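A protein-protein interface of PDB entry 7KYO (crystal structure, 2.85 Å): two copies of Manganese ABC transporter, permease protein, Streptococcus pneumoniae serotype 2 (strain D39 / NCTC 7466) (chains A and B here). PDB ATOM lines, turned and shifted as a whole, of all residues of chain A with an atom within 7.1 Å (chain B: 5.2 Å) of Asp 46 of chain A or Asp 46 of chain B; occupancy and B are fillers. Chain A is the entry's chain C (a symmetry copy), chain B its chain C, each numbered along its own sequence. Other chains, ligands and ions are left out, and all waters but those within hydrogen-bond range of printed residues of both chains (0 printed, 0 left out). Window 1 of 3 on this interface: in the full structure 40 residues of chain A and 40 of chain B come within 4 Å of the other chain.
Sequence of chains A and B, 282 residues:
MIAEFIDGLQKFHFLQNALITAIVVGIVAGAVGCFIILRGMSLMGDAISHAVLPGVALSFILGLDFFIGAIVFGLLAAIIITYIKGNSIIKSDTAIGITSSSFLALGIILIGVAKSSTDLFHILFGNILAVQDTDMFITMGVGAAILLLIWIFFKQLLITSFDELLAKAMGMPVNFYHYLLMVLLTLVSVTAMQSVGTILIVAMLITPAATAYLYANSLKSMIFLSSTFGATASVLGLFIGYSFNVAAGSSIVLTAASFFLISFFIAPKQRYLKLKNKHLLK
Of the printed residues of chain B, Leu 43 of chain A touches Leu 43 (3.2 Å). Of the printed residues of chain B, Asp 46 of chain A touches Asp 46 (3.5 Å). Printed residues of chain B within 4 Å of Ile 199 of chain A: Ile 199. Printed residues of chain A within 4 Å of Leu 43 of chain B: Leu 43. No residue of chain A comes within 4 Å of Gly 45 of chain B. Of chain A, only Asp 46 comes within 4 Å of Asp 46 of chain B. Of the printed residues of chain A, Ile 199 of chain B touches Ile 199 (3.7 Å). The nearest printed residue of chain B that does not touch Asp 46 of chain A is His 50 of chain B (5.8 Å). The nearest printed residue of chain A that does not touch Ile 199 of chain B is His 50 of chain A (5.3 Å).
Leu 43 of chain B touches its own counterpart, Leu 43 of chain A. Asp 46 of chain A touches its own counterpart, Asp 46 of chain B. Ile 199 of chain A touches its own counterpart, Ile 199 of chain B. 11 positions are printed for both chains. Of the 3 pairs that touch across the chains among the printed residues, 3 have their exchanged pair printed and touching as well.
O of Asp 46 of chain B sits at hydrogen-bond distance from ND1 of His 50 of chain B (3.0 Å). A ring nitrogen (ND1) of His 50 of chain A lies within hydrogen-bond range of the backbone carbonyl oxygen (O) of Asp 46 of chain A.
Hydrophobic or aromatic side chains of chain A that line the printed part of chain B: Leu 43 and Ile 199. Of the 11 printed residues of chain B, 3 touch a printed residue of chain A. Hydrophobic or aromatic side chains of chain B within 4 Å of the printed part of chain A: Leu 43 and Ile 199. Among the printed residues, 3 pairs touch across the chains.
The side-chain carboxylate (OD2) of Asp 46 of chain B sits close to the side-chain carboxylate (OD2) of Asp 46 of chain A, 3.5 Å away.
CD1 of Leu 43 of chain A touches CD1 of Leu 43 of chain B (3.2 Å). Ile 199 of chain A touches Ile 199 of chain B.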
ATOM      1  N   MET A  41      -8.378  -0.732 -25.897  1.00  0.00           N
ATOM      2  CA  MET A  41      -7.652  -1.910 -25.413  1.00  0.00           C
ATOM      3  C   MET A  41      -6.499  -2.288 -26.356  1.00  0.00           C
ATOM      4  O   MET A  41      -6.017  -3.421 -26.316  1.00  0.00           O
ATOM      5  CB  MET A  41      -8.622  -3.096 -25.275  1.00  0.00           C
ATOM      6  CG  MET A  41      -9.782  -2.878 -24.314  1.00  0.00           C
ATOM      7  SD  MET A  41     -11.044  -4.169 -24.428  1.00  0.00           S
ATOM      8  CE  MET A  41     -10.135  -5.607 -23.870  1.00  0.00           C
ATOM      9  N   SER A  42      -6.048  -1.344 -27.188  1.00  0.00           N
ATOM     10  CA  SER A  42      -5.022  -1.616 -28.206  1.00  0.00           C
ATOM     11  C   SER A  42      -3.661  -1.987 -27.613  1.00  0.00           C
ATOM     12  O   SER A  42      -2.942  -2.812 -28.181  1.00  0.00           O
ATOM     13  CB  SER A  42      -4.861  -0.414 -29.142  1.00  0.00           C
ATOM     14  OG  SER A  42      -4.423   0.732 -28.431  1.00  0.00           O
ATOM     15  N   LEU A  43      -3.322  -1.384 -26.475  1.00  0.00           N
ATOM     16  CA  LEU A  43      -2.057  -1.660 -25.779  1.00  0.00           C
ATOM     17  C   LEU A  43      -2.139  -2.921 -24.909  1.00  0.00           C
ATOM     18  O   LEU A  43      -1.106  -3.474 -24.529  1.00  0.00           O
ATOM     19  CB  LEU A  43      -1.626  -0.446 -24.944  1.00  0.00           C
ATOM     20  CG  LEU A  43      -1.669   0.920 -25.655  1.00  0.00           C
ATOM     21  CD1 LEU A  43      -1.001   1.995 -24.811  1.00  0.00           C
ATOM     22  CD2 LEU A  43      -1.033   0.863 -27.038  1.00  0.00           C
ATOM     23  N   MET A  44      -3.360  -3.357 -24.588  1.00  0.00           N
ATOM     24  CA  MET A  44      -3.601  -4.678 -23.995  1.00  0.00           C
ATOM     25  C   MET A  44      -3.607  -5.787 -25.057  1.00  0.00           C
ATOM     26  O   MET A  44      -3.251  -6.928 -24.759  1.00  0.00           O
ATOM     27  CB  MET A  44      -4.926  -4.692 -23.234  1.00  0.00           C
ATOM     28  CG  MET A  44      -5.053  -5.844 -22.250  1.00  0.00           C
ATOM     29  SD  MET A  44      -6.650  -5.892 -21.419  1.00  0.00           S
ATOM     30  CE  MET A  44      -6.650  -4.325 -20.544  1.00  0.00           C
ATOM     31  N   GLY A  45      -4.029  -5.455 -26.279  1.00  0.00           N
ATOM     32  CA  GLY A  45      -3.965  -6.380 -27.417  1.00  0.00           C
ATOM     33  C   GLY A  45      -2.558  -6.779 -27.847  1.00  0.00           C
ATOM     34  O   GLY A  45      -2.377  -7.814 -28.492  1.00  0.00           O
ATOM     35  N   ASP A  46      -1.570  -5.949 -27.514  1.00  0.00           N
ATOM     36  CA  ASP A  46      -0.156  -6.277 -27.713  1.00  0.00           C
ATOM     37  C   ASP A  46       0.327  -7.282 -26.662  1.00  0.00           C
ATOM     38  O   ASP A  46       0.963  -8.282 -27.001  1.00  0.00           O
ATOM     39  CB  ASP A  46       0.690  -4.997 -27.657  1.00  0.00           C
ATOM     40  CG  ASP A  46       2.117  -5.205 -28.148  1.00  0.00           C
ATOM     41  OD1 ASP A  46       2.300  -5.669 -29.294  1.00  0.00           O
ATOM     42  OD2 ASP A  46       3.059  -4.885 -27.389  1.00  0.00           O
ATOM     43  N   ALA A  47       0.010  -7.008 -25.396  1.00  0.00           N
ATOM     44  CA  ALA A  47       0.473  -7.824 -24.264  1.00  0.00           C
ATOM     45  C   ALA A  47      -0.111  -9.239 -24.232  1.00  0.00           C
ATOM     46  O   ALA A  47       0.585 -10.185 -23.857  1.00  0.00           O
ATOM     47  CB  ALA A  47       0.178  -7.113 -22.949  1.00  0.00           C
ATOM     48  N   ILE A  48      -1.383  -9.374 -24.609  1.00  0.00           N
ATOM     49  CA  ILE A  48      -2.053 -10.685 -24.669  1.00  0.00           C
ATOM     50  C   ILE A  48      -1.404 -11.636 -25.684  1.00  0.00           C
ATOM     51  O   ILE A  48      -1.402 -12.850 -25.486  1.00  0.00           O
ATOM     52  CB  ILE A  48      -3.571 -10.539 -24.969  1.00  0.00           C
ATOM     53  CG1 ILE A  48      -4.324 -11.838 -24.658  1.00  0.00           C
ATOM     54  CG2 ILE A  48      -3.827 -10.110 -26.413  1.00  0.00           C
ATOM     55  CD1 ILE A  48      -5.829 -11.694 -24.730  1.00  0.00           C
ATOM     56  N   SER A  49      -0.856 -11.069 -26.757  1.00  0.00           N
ATOM     57  CA  SER A  49      -0.190 -11.836 -27.806  1.00  0.00           C
ATOM     58  C   SER A  49       1.124 -12.444 -27.333  1.00  0.00           C
ATOM     59  O   SER A  49       1.440 -13.585 -27.671  1.00  0.00           O
ATOM     60  CB  SER A  49       0.078 -10.938 -29.007  1.00  0.00           C
ATOM     61  OG  SER A  49      -1.086 -10.201 -29.338  1.00  0.00           O
ATOM     62  N   HIS A  50       1.890 -11.671 -26.568  1.00  0.00           N
ATOM     63  CA  HIS A  50       3.130 -12.159 -25.961  1.00  0.00           C
ATOM     64  C   HIS A  50       2.854 -13.163 -24.834  1.00  0.00           C
ATOM     65  O   HIS A  50       3.627 -14.103 -24.637  1.00  0.00           O
ATOM     66  CB  HIS A  50       3.971 -10.994 -25.429  1.00  0.00           C
ATOM     67  CG  HIS A  50       4.391 -10.020 -26.485  1.00  0.00           C
ATOM     68  ND1 HIS A  50       3.850  -8.757 -26.591  1.00  0.00           N
ATOM     69  CD2 HIS A  50       5.293 -10.127 -27.488  1.00  0.00           C
ATOM     70  CE1 HIS A  50       4.405  -8.126 -27.611  1.00  0.00           C
ATOM     71  NE2 HIS A  50       5.284  -8.936 -28.171  1.00  0.00           N
ATOM     72  N   ALA A  51       1.754 -12.960 -24.107  1.00  0.00           N
ATOM     73  CA  ALA A  51       1.355 -13.849 -23.009  1.00  0.00           C
ATOM     74  C   ALA A  51       0.943 -15.255 -23.465  1.00  0.00           C
ATOM     75  O   ALA A  51       1.162 -16.226 -22.738  1.00  0.00           O
ATOM     76  CB  ALA A  51       0.230 -13.213 -22.205  1.00  0.00           C
ATOM     77  N   ILE A  96       2.433  -4.745 -16.888  1.00  0.00           N
ATOM     78  CA  ILE A  96       2.028  -5.387 -18.148  1.00  0.00           C
ATOM     79  C   ILE A  96       3.252  -5.587 -19.046  1.00  0.00           C
ATOM     80  O   ILE A  96       3.387  -6.632 -19.683  1.00  0.00           O
ATOM     81  CB  ILE A  96       0.952  -4.566 -18.905  1.00  0.00           C
ATOM     82  CG1 ILE A  96      -0.357  -4.512 -18.104  1.00  0.00           C
ATOM     83  CG2 ILE A  96       0.669  -5.164 -20.283  1.00  0.00           C
ATOM     84  CD1 ILE A  96      -1.289  -3.389 -18.511  1.00  0.00           C
ATOM     85  N   SER A 100       4.609  -9.352 -20.104  1.00  0.00           N
ATOM     86  CA  SER A 100       4.496  -9.635 -21.538  1.00  0.00           C
ATOM     87  C   SER A 100       5.858  -9.978 -22.142  1.00  0.00           C
ATOM     88  O   SER A 100       6.004 -11.000 -22.813  1.00  0.00           O
ATOM     89  CB  SER A 100       3.879  -8.449 -22.283  1.00  0.00           C
ATOM     90  OG  SER A 100       4.745  -7.327 -22.267  1.00  0.00           O
ATOM     91  N   SER A 101       6.846  -9.122 -21.890  1.00  0.00           N
ATOM     92  CA  SER A 101       8.211  -9.320 -22.397  1.00  0.00           C
ATOM     93  C   SER A 101       8.894 -10.554 -21.810  1.00  0.00           C
ATOM     94  O   SER A 101       9.621 -11.253 -22.517  1.00  0.00           O
ATOM     95  CB  SER A 101       9.070  -8.083 -22.121  1.00  0.00           C
ATOM     96  OG  SER A 101       8.517  -6.934 -22.739  1.00  0.00           O
ATOM     97  N   LEU A 185     -10.699 -12.334 -27.917  1.00  0.00           N
ATOM     98  CA  LEU A 185      -9.374 -11.808 -28.272  1.00  0.00           C
ATOM     99  C   LEU A 185      -8.257 -12.865 -28.236  1.00  0.00           C
ATOM    100  O   LEU A 185      -7.358 -12.825 -29.072  1.00  0.00           O
ATOM    101  CB  LEU A 185      -9.012 -10.621 -27.364  1.00  0.00           C
ATOM    102  CG  LEU A 185      -7.687  -9.886 -27.608  1.00  0.00           C
ATOM    103  CD1 LEU A 185      -7.499  -9.493 -29.070  1.00  0.00           C
ATOM    104  CD2 LEU A 185      -7.604  -8.667 -26.704  1.00  0.00           C
ATOM    105  N   THR A 198       2.917 -13.775 -34.104  1.00  0.00           N
ATOM    106  CA  THR A 198       2.654 -13.101 -32.822  1.00  0.00           C
ATOM    107  C   THR A 198       3.149 -11.654 -32.772  1.00  0.00           C
ATOM    108  O   THR A 198       2.605 -10.846 -32.020  1.00  0.00           O
ATOM    109  CB  THR A 198       3.281 -13.853 -31.626  1.00  0.00           C
ATOM    110  OG1 THR A 198       4.707 -13.887 -31.760  1.00  0.00           O
ATOM    111  CG2 THR A 198       2.745 -15.270 -31.532  1.00  0.00           C
ATOM    112  N   ILE A 199       4.177 -11.337 -33.558  1.00  0.00           N
ATOM    113  CA  ILE A 199       4.801 -10.009 -33.534  1.00  0.00           C
ATOM    114  C   ILE A 199       3.907  -8.955 -34.197  1.00  0.00           C
ATOM    115  O   ILE A 199       3.649  -7.906 -33.607  1.00  0.00           O
ATOM    116  CB  ILE A 199       6.206 -10.033 -34.187  1.00  0.00           C
ATOM    117  CG1 ILE A 199       7.151 -10.927 -33.372  1.00  0.00           C
ATOM    118  CG2 ILE A 199       6.791  -8.626 -34.300  1.00  0.00           C
ATOM    119  CD1 ILE A 199       8.362 -11.410 -34.142  1.00  0.00           C
ATOM    120  N   ILE A 201       0.671  -9.319 -35.064  1.00  0.00           N
ATOM    121  CA  ILE A 201      -0.752  -9.601 -34.784  1.00  0.00           C
ATOM    122  C   ILE A 201      -1.622  -8.384 -34.433  1.00  0.00           C
ATOM    123  O   ILE A 201      -2.821  -8.377 -34.728  1.00  0.00           O
ATOM    124  CB  ILE A 201      -0.869 -10.630 -33.638  1.00  0.00           C
ATOM    125  CG1 ILE A 201      -2.282 -11.201 -33.533  1.00  0.00           C
ATOM    126  CG2 ILE A 201      -0.426 -10.028 -32.309  1.00  0.00           C
ATOM    127  CD1 ILE A 201      -2.351 -12.415 -32.639  1.00  0.00           C
ATOM    128  N   VAL A 202      -1.022  -7.375 -33.804  1.00  0.00           N
ATOM    129  CA  VAL A 202      -1.756  -6.194 -33.332  1.00  0.00           C
ATOM    130  C   VAL A 202      -2.317  -5.404 -34.512  1.00  0.00           C
ATOM    131  O   VAL A 202      -3.446  -4.916 -34.448  1.00  0.00           O
ATOM    132  CB  VAL A 202      -0.873  -5.270 -32.459  1.00  0.00           C
ATOM    133  CG1 VAL A 202      -1.660  -4.048 -31.985  1.00  0.00           C
ATOM    134  CG2 VAL A 202      -0.310  -6.042 -31.272  1.00  0.00           C
ATOM    135  N   LEU A 205      -5.690  -6.512 -35.818  1.00  0.00           N
ATOM    136  CA  LEU A 205      -6.798  -6.029 -34.999  1.00  0.00           C
ATOM    137  C   LEU A 205      -7.078  -4.549 -35.278  1.00  0.00           C
ATOM    138  O   LEU A 205      -8.157  -4.200 -35.762  1.00  0.00           O
ATOM    139  CB  LEU A 205      -6.502  -6.243 -33.510  1.00  0.00           C
ATOM    140  CG  LEU A 205      -6.278  -7.695 -33.071  1.00  0.00           C
ATOM    141  CD1 LEU A 205      -5.732  -7.745 -31.651  1.00  0.00           C
ATOM    142  CD2 LEU A 205      -7.560  -8.509 -33.183  1.00  0.00           C
ATOM    143  N   SER B  42       6.624   3.704 -20.687  1.00  0.00           N
ATOM    144  CA  SER B  42       6.951   2.308 -21.010  1.00  0.00           C
ATOM    145  C   SER B  42       6.293   1.811 -22.298  1.00  0.00           C
ATOM    146  O   SER B  42       6.886   1.017 -23.031  1.00  0.00           O
ATOM    147  CB  SER B  42       6.565   1.384 -19.850  1.00  0.00           C
ATOM    148  OG  SER B  42       5.168   1.421 -19.611  1.00  0.00           O
ATOM    149  N   LEU B  43       5.079   2.287 -22.570  1.00  0.00           N
ATOM    150  CA  LEU B  43       4.337   1.919 -23.784  1.00  0.00           C
ATOM    151  C   LEU B  43       4.768   2.749 -25.000  1.00  0.00           C
ATOM    152  O   LEU B  43       4.499   2.358 -26.137  1.00  0.00           O
ATOM    153  CB  LEU B  43       2.824   2.039 -23.547  1.00  0.00           C
ATOM    154  CG  LEU B  43       2.283   1.394 -22.257  1.00  0.00           C
ATOM    155  CD1 LEU B  43       0.762   1.372 -22.257  1.00  0.00           C
ATOM    156  CD2 LEU B  43       2.832  -0.012 -22.049  1.00  0.00           C
ATOM    157  N   MET B  44       5.418   3.889 -24.755  1.00  0.00           N
ATOM    158  CA  MET B  44       6.116   4.645 -25.801  1.00  0.00           C
ATOM    159  C   MET B  44       7.500   4.054 -26.106  1.00  0.00           C
ATOM    160  O   MET B  44       7.983   4.160 -27.234  1.00  0.00           O
ATOM    161  CB  MET B  44       6.265   6.112 -25.396  1.00  0.00           C
ATOM    162  CG  MET B  44       6.574   7.039 -26.561  1.00  0.00           C
ATOM    163  SD  MET B  44       6.824   8.750 -26.057  1.00  0.00           S
ATOM    164  CE  MET B  44       5.226   9.155 -25.349  1.00  0.00           C
ATOM    165  N   GLY B  45       8.139   3.455 -25.098  1.00  0.00           N
ATOM    166  CA  GLY B  45       9.406   2.736 -25.279  1.00  0.00           C
ATOM    167  C   GLY B  45       9.326   1.498 -26.163  1.00  0.00           C
ATOM    168  O   GLY B  45      10.342   1.056 -26.704  1.00  0.00           O
ATOM    169  N   ASP B  46       8.128   0.926 -26.290  1.00  0.00           N
ATOM    170  CA  ASP B  46       7.865  -0.165 -27.231  1.00  0.00           C
ATOM    171  C   ASP B  46       7.771   0.359 -28.667  1.00  0.00           C
ATOM    172  O   ASP B  46       8.394  -0.194 -29.575  1.00  0.00           O
ATOM    173  CB  ASP B  46       6.568  -0.890 -26.840  1.00  0.00           C
ATOM    174  CG  ASP B  46       6.380  -2.209 -27.576  1.00  0.00           C
ATOM    175  OD1 ASP B  46       7.276  -3.078 -27.500  1.00  0.00           O
ATOM    176  OD2 ASP B  46       5.321  -2.385 -28.219  1.00  0.00           O
ATOM    177  N   ALA B  47       6.998   1.430 -28.853  1.00  0.00           N
ATOM    178  CA  ALA B  47       6.734   2.001 -30.182  1.00  0.00           C
ATOM    179  C   ALA B  47       7.963   2.620 -30.853  1.00  0.00           C
ATOM    180  O   ALA B  47       8.119   2.515 -32.072  1.00  0.00           O
ATOM    181  CB  ALA B  47       5.617   3.034 -30.097  1.00  0.00           C
ATOM    182  N   ILE B  48       8.818   3.269 -30.063  1.00  0.00           N
ATOM    183  CA  ILE B  48      10.063   3.871 -30.573  1.00  0.00           C
ATOM    184  C   ILE B  48      11.027   2.831 -31.157  1.00  0.00           C
ATOM    185  O   ILE B  48      11.770   3.126 -32.092  1.00  0.00           O
ATOM    186  CB  ILE B  48      10.782   4.712 -29.480  1.00  0.00           C
ATOM    187  CG1 ILE B  48      11.844   5.629 -30.098  1.00  0.00           C
ATOM    188  CG2 ILE B  48      11.406   3.829 -28.402  1.00  0.00           C
ATOM    189  CD1 ILE B  48      12.429   6.620 -29.114  1.00  0.00           C
ATOM    190  N   SER B  49      11.000   1.622 -30.599  1.00  0.00           N
ATOM    191  CA  SER B  49      11.847   0.520 -31.050  1.00  0.00           C
ATOM    192  C   SER B  49      11.443   0.005 -32.425  1.00  0.00           C
ATOM    193  O   SER B  49      12.302  -0.304 -33.251  1.00  0.00           O
ATOM    194  CB  SER B  49      11.778  -0.623 -30.046  1.00  0.00           C
ATOM    195  OG  SER B  49      11.947  -0.131 -28.728  1.00  0.00           O
ATOM    196  N   HIS B  50      10.137  -0.101 -32.655  1.00  0.00           N
ATOM    197  CA  HIS B  50       9.605  -0.487 -33.963  1.00  0.00           C
ATOM    198  C   HIS B  50       9.794   0.625 -35.003  1.00  0.00           C
ATOM    199  O   HIS B  50      10.012   0.341 -36.183  1.00  0.00           O
ATOM    200  CB  HIS B  50       8.123  -0.861 -33.860  1.00  0.00           C
ATOM    201  CG  HIS B  50       7.854  -2.021 -32.953  1.00  0.00           C
ATOM    202  ND1 HIS B  50       7.257  -1.879 -31.720  1.00  0.00           N
ATOM    203  CD2 HIS B  50       8.109  -3.342 -33.097  1.00  0.00           C
ATOM    204  CE1 HIS B  50       7.151  -3.064 -31.145  1.00  0.00           C
ATOM    205  NE2 HIS B  50       7.660  -3.968 -31.960  1.00  0.00           N
ATOM    206  N   ILE B 199      12.872  -6.633 -30.642  1.00  0.00           N
ATOM    207  CA  ILE B 199      11.656  -7.230 -30.079  1.00  0.00           C
ATOM    208  C   ILE B 199      11.673  -7.201 -28.546  1.00  0.00           C
ATOM    209  O   ILE B 199      10.711  -6.745 -27.928  1.00  0.00           O
ATOM    210  CB  ILE B 199      11.439  -8.672 -30.602  1.00  0.00           C
ATOM    211  CG1 ILE B 199      11.201  -8.652 -32.119  1.00  0.00           C
ATOM    212  CG2 ILE B 199      10.260  -9.346 -29.901  1.00  0.00           C
ATOM    213  CD1 ILE B 199      11.457  -9.978 -32.802  1.00  0.00           C
ATOM    214  N   VAL B 202      12.453  -3.663 -24.829  1.00  0.00           N
ATOM    215  CA  VAL B 202      11.671  -2.971 -23.797  1.00  0.00           C
ATOM    216  C   VAL B 202      12.022  -3.503 -22.410  1.00  0.00           C
ATOM    217  O   VAL B 202      12.128  -2.727 -21.459  1.00  0.00           O
ATOM    218  CB  VAL B 202      10.147  -3.104 -24.035  1.00  0.00           C
ATOM    219  CG1 VAL B 202       9.356  -2.379 -22.946  1.00  0.00           C
ATOM    220  CG2 VAL B 202       9.778  -2.572 -25.415  1.00  0.00           C
